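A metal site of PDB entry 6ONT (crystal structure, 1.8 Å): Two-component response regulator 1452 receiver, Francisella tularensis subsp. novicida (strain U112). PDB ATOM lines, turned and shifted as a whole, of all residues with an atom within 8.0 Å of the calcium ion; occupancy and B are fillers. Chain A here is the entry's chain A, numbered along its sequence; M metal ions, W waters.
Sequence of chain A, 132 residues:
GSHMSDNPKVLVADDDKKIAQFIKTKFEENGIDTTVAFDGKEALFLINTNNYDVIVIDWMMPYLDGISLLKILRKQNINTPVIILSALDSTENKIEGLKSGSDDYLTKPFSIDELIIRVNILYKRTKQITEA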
ATOM      1  N   ALA A  13      10.636  28.229 -19.986  1.00  0.00           N
ATOM      2  CA  ALA A  13      10.232  28.582 -21.345  1.00  0.00           C
ATOM      3  C   ALA A  13       8.757  28.959 -21.367  1.00  0.00           C
ATOM      4  O   ALA A  13       7.888  28.108 -21.132  1.00  0.00           O
ATOM      5  CB  ALA A  13      10.514  27.422 -22.305  1.00  0.00           C
ATOM      6  N   ASP A  14       8.477  30.231 -21.640  1.00  0.00           N
ATOM      7  CA  ASP A  14       7.127  30.663 -21.959  1.00  0.00           C
ATOM      8  C   ASP A  14       7.205  31.926 -22.805  1.00  0.00           C
ATOM      9  O   ASP A  14       8.111  32.743 -22.623  1.00  0.00           O
ATOM     10  CB  ASP A  14       6.280  30.895 -20.713  1.00  0.00           C
ATOM     11  CG  ASP A  14       4.799  31.024 -21.036  1.00  0.00           C
ATOM     12  OD1 ASP A  14       4.423  30.708 -22.188  1.00  0.00           O
ATOM     13  OD2 ASP A  14       4.017  31.445 -20.159  1.00  0.00           O
ATOM     14  N   ASP A  15       6.234  32.110 -23.693  1.00  0.00           N
ATOM     15  CA  ASP A  15       6.183  33.315 -24.509  1.00  0.00           C
ATOM     16  C   ASP A  15       5.433  34.461 -23.828  1.00  0.00           C
ATOM     17  O   ASP A  15       5.489  35.589 -24.329  1.00  0.00           O
ATOM     18  CB  ASP A  15       5.545  33.014 -25.878  1.00  0.00           C
ATOM     19  CG  ASP A  15       4.128  32.445 -25.769  1.00  0.00           C
ATOM     20  OD1 ASP A  15       3.829  31.778 -24.763  1.00  0.00           O
ATOM     21  OD2 ASP A  15       3.308  32.662 -26.687  1.00  0.00           O
ATOM     22  N   ASP A  16       4.770  34.219 -22.698  1.00  0.00           N
ATOM     23  CA  ASP A  16       4.118  35.271 -21.928  1.00  0.00           C
ATOM     24  C   ASP A  16       5.167  35.925 -21.041  1.00  0.00           C
ATOM     25  O   ASP A  16       5.575  35.366 -20.025  1.00  0.00           O
ATOM     26  CB  ASP A  16       2.972  34.695 -21.109  1.00  0.00           C
ATOM     27  CG  ASP A  16       2.185  35.770 -20.365  1.00  0.00           C
ATOM     28  OD1 ASP A  16       2.810  36.667 -19.764  1.00  0.00           O
ATOM     29  OD2 ASP A  16       0.940  35.700 -20.387  1.00  0.00           O
ATOM     30  N   LYS A  17       5.629  37.111 -21.432  1.00  0.00           N
ATOM     31  CA  LYS A  17       6.777  37.717 -20.761  1.00  0.00           C
ATOM     32  C   LYS A  17       6.464  38.088 -19.315  1.00  0.00           C
ATOM     33  O   LYS A  17       7.354  38.030 -18.459  1.00  0.00           O
ATOM     34  CB  LYS A  17       7.233  38.942 -21.542  1.00  0.00           C
ATOM     35  CG  LYS A  17       7.811  38.632 -22.922  1.00  0.00           C
ATOM     36  CD  LYS A  17       8.176  39.923 -23.641  1.00  0.00           C
ATOM     37  CE  LYS A  17       8.820  39.646 -24.986  1.00  0.00           C
ATOM     38  NZ  LYS A  17       9.049  40.917 -25.726  1.00  0.00           N
ATOM     39  N   ILE A  19       4.404  36.446 -17.214  1.00  0.00           N
ATOM     40  CA  ILE A  19       4.452  35.210 -16.437  1.00  0.00           C
ATOM     41  C   ILE A  19       5.895  34.716 -16.294  1.00  0.00           C
ATOM     42  O   ILE A  19       6.312  34.284 -15.215  1.00  0.00           O
ATOM     43  CB  ILE A  19       3.553  34.129 -17.085  1.00  0.00           C
ATOM     44  CG1 ILE A  19       2.085  34.532 -17.005  1.00  0.00           C
ATOM     45  CG2 ILE A  19       3.796  32.784 -16.408  1.00  0.00           C
ATOM     46  CD1 ILE A  19       1.484  34.367 -15.625  1.00  0.00           C
ATOM     47  N   PHE A  38      11.867  32.574 -24.534  1.00  0.00           N
ATOM     48  CA  PHE A  38      10.552  33.098 -24.861  1.00  0.00           C
ATOM     49  C   PHE A  38       9.837  32.370 -25.986  1.00  0.00           C
ATOM     50  O   PHE A  38       8.733  32.769 -26.369  1.00  0.00           O
ATOM     51  CB  PHE A  38      10.629  34.587 -25.191  1.00  0.00           C
ATOM     52  CG  PHE A  38      10.944  35.437 -24.007  1.00  0.00           C
ATOM     53  CD1 PHE A  38      10.087  35.477 -22.915  1.00  0.00           C
ATOM     54  CD2 PHE A  38      12.097  36.217 -23.970  1.00  0.00           C
ATOM     55  CE1 PHE A  38      10.369  36.256 -21.824  1.00  0.00           C
ATOM     56  CE2 PHE A  38      12.387  36.998 -22.874  1.00  0.00           C
ATOM     57  CZ  PHE A  38      11.510  37.022 -21.802  1.00  0.00           C
ATOM     58  N   ILE A  57       8.406  24.115 -18.745  1.00  0.00           N
ATOM     59  CA  ILE A  57       7.986  24.345 -20.114  1.00  0.00           C
ATOM     60  C   ILE A  57       6.502  24.678 -20.160  1.00  0.00           C
ATOM     61  O   ILE A  57       5.673  23.905 -19.655  1.00  0.00           O
ATOM     62  CB  ILE A  57       8.275  23.127 -21.012  1.00  0.00           C
ATOM     63  CG1 ILE A  57       9.744  22.716 -20.941  1.00  0.00           C
ATOM     64  CG2 ILE A  57       7.850  23.438 -22.437  1.00  0.00           C
ATOM     65  CD1 ILE A  57      10.036  21.472 -21.767  1.00  0.00           C
ATOM     66  N   ASP A  58       6.159  25.803 -20.792  1.00  0.00           N
ATOM     67  CA  ASP A  58       4.767  26.150 -21.032  1.00  0.00           C
ATOM     68  C   ASP A  58       4.204  25.362 -22.208  1.00  0.00           C
ATOM     69  O   ASP A  58       4.926  25.038 -23.159  1.00  0.00           O
ATOM     70  CB  ASP A  58       4.611  27.646 -21.287  1.00  0.00           C
ATOM     71  CG  ASP A  58       3.152  28.063 -21.403  1.00  0.00           C
ATOM     72  OD1 ASP A  58       2.669  28.319 -22.524  1.00  0.00           O
ATOM     73  OD2 ASP A  58       2.479  28.087 -20.357  1.00  0.00           O
ATOM     74  N   TRP A  59       2.896  25.093 -22.157  1.00  0.00           N
ATOM     75  CA  TRP A  59       2.295  24.162 -23.103  1.00  0.00           C
ATOM     76  C   TRP A  59       2.215  24.743 -24.508  1.00  0.00           C
ATOM     77  O   TRP A  59       2.181  23.983 -25.479  1.00  0.00           O
ATOM     78  CB  TRP A  59       0.899  23.746 -22.646  1.00  0.00           C
ATOM     79  CG  TRP A  59      -0.119  24.820 -22.762  1.00  0.00           C
ATOM     80  CD1 TRP A  59      -0.156  25.990 -22.055  1.00  0.00           C
ATOM     81  CD2 TRP A  59      -1.232  24.847 -23.647  1.00  0.00           C
ATOM     82  NE1 TRP A  59      -1.237  26.742 -22.456  1.00  0.00           N
ATOM     83  CE2 TRP A  59      -1.907  26.064 -23.436  1.00  0.00           C
ATOM     84  CE3 TRP A  59      -1.727  23.972 -24.621  1.00  0.00           C
ATOM     85  CZ2 TRP A  59      -3.054  26.429 -24.147  1.00  0.00           C
ATOM     86  CZ3 TRP A  59      -2.873  24.341 -25.315  1.00  0.00           C
ATOM     87  CH2 TRP A  59      -3.523  25.546 -25.079  1.00  0.00           C
ATOM     88  N   MET A  60       2.163  26.065 -24.643  1.00  0.00           N
ATOM     89  CA  MET A  60       2.001  26.675 -25.959  1.00  0.00           C
ATOM     90  C   MET A  60       2.913  27.881 -26.125  1.00  0.00           C
ATOM     91  O   MET A  60       2.811  28.863 -25.391  1.00  0.00           O
ATOM     92  CB  MET A  60       0.537  27.071 -26.159  1.00  0.00           C
ATOM     93  CG  MET A  60       0.171  27.478 -27.594  1.00  0.00           C
ATOM     94  SD  MET A  60       0.708  26.352 -28.904  1.00  0.00           S
ATOM     95  CE  MET A  60      -0.062  24.845 -28.339  1.00  0.00           C
ATOM     96  N   MET A  61       3.773  27.795 -27.134  1.00  0.00           N
ATOM     97  CA  MET A  61       4.686  28.875 -27.489  1.00  0.00           C
ATOM     98  C   MET A  61       4.959  28.810 -28.984  1.00  0.00           C
ATOM     99  O   MET A  61       4.701  27.782 -29.621  1.00  0.00           O
ATOM    100  CB  MET A  61       6.013  28.766 -26.730  1.00  0.00           C
ATOM    101  CG  MET A  61       5.966  28.186 -25.353  1.00  0.00           C
ATOM    102  SD  MET A  61       7.675  27.975 -24.800  1.00  0.00           S
ATOM    103  CE  MET A  61       7.980  26.242 -25.087  1.00  0.00           C
ATOM    104  N   PRO A  62       5.536  29.870 -29.555  1.00  0.00           N
ATOM    105  CA  PRO A  62       5.883  29.826 -30.983  1.00  0.00           C
ATOM    106  C   PRO A  62       6.936  28.759 -31.295  1.00  0.00           C
ATOM    107  O   PRO A  62       7.727  28.361 -30.437  1.00  0.00           O
ATOM    108  CB  PRO A  62       6.421  31.235 -31.268  1.00  0.00           C
ATOM    109  CG  PRO A  62       5.799  32.105 -30.198  1.00  0.00           C
ATOM    110  CD  PRO A  62       5.661  31.221 -28.983  1.00  0.00           C
ATOM    111  N   LEU A  85       3.712  23.267 -17.680  1.00  0.00           N
ATOM    112  CA  LEU A  85       2.655  24.169 -17.249  1.00  0.00           C
ATOM    113  C   LEU A  85       1.627  24.229 -18.370  1.00  0.00           C
ATOM    114  O   LEU A  85       1.960  24.639 -19.487  1.00  0.00           O
ATOM    115  CB  LEU A  85       3.175  25.568 -16.945  1.00  0.00           C
ATOM    116  CG  LEU A  85       4.380  25.662 -16.013  1.00  0.00           C
ATOM    117  CD1 LEU A  85       4.817  27.128 -15.893  1.00  0.00           C
ATOM    118  CD2 LEU A  85       4.099  25.066 -14.632  1.00  0.00           C
ATOM    119  N   LYS A 108      -2.916  25.442 -15.188  1.00  0.00           N
ATOM    120  CA  LYS A 108      -2.990  26.884 -14.988  1.00  0.00           C
ATOM    121  C   LYS A 108      -4.429  27.297 -14.669  1.00  0.00           C
ATOM    122  O   LYS A 108      -5.371  26.742 -15.248  1.00  0.00           O
ATOM    123  CB  LYS A 108      -2.502  27.613 -16.238  1.00  0.00           C
ATOM    124  CG  LYS A 108      -1.134  27.143 -16.717  1.00  0.00           C
ATOM    125  CD  LYS A 108      -0.911  27.503 -18.183  1.00  0.00           C
ATOM    126  CE  LYS A 108       0.231  28.480 -18.363  1.00  0.00           C
ATOM    127  NZ  LYS A 108       0.002  29.398 -19.512  1.00  0.00           N
HETATM  128 CA    CA M   1       2.292  30.382 -23.585  1.00  0.00          CA
HETATM  129  O   HOH W   1       0.088  30.034 -24.093  1.00  0.00           O
HETATM  130  O   HOH W   2       1.221  32.722 -23.697  1.00  0.00           O
HETATM  131  O   HOH W   3       1.627  31.249 -21.288  1.00  0.00           O
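Water W3 lies within hydrogen-bond range of the side-chain carboxylate (OD2) of Asp 14 (2.7 Å), the side-chain amino group (NZ) of Lys 108 (3.0 Å) and the side-chain carboxylate (OD2) of Asp 58 (3.4 Å).
Within 4 Å of the calcium ion: Asp 14, Asp 15, Asp 58 and Met 60. The nearest printed residue that does not touch the calcium ion is Met 61 (4.6 Å).
The side-chain carboxylate (OD2) of Asp 58 is in salt-bridge range of the side-chain amino group (NZ) of Lys 108. The backbone NH (N) of Asp 58 lies within hydrogen-bond range of the backbone carbonyl oxygen (O) of Ala 13.
The calcium ion is bound by water W1 (2.3 Å), the side-chain carboxylate of Asp 58 (2.4 Å), the side-chain carboxylate of Asp 15 (2.4 Å), the backbone carbonyl oxygen of Met 60 (2.4 Å), water W3 (2.5 Å), the side-chain carboxylate of Asp 14 (2.6 Å) and water W2 (2.6 Å). The calcium ion has seven donor atoms within binding distance.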
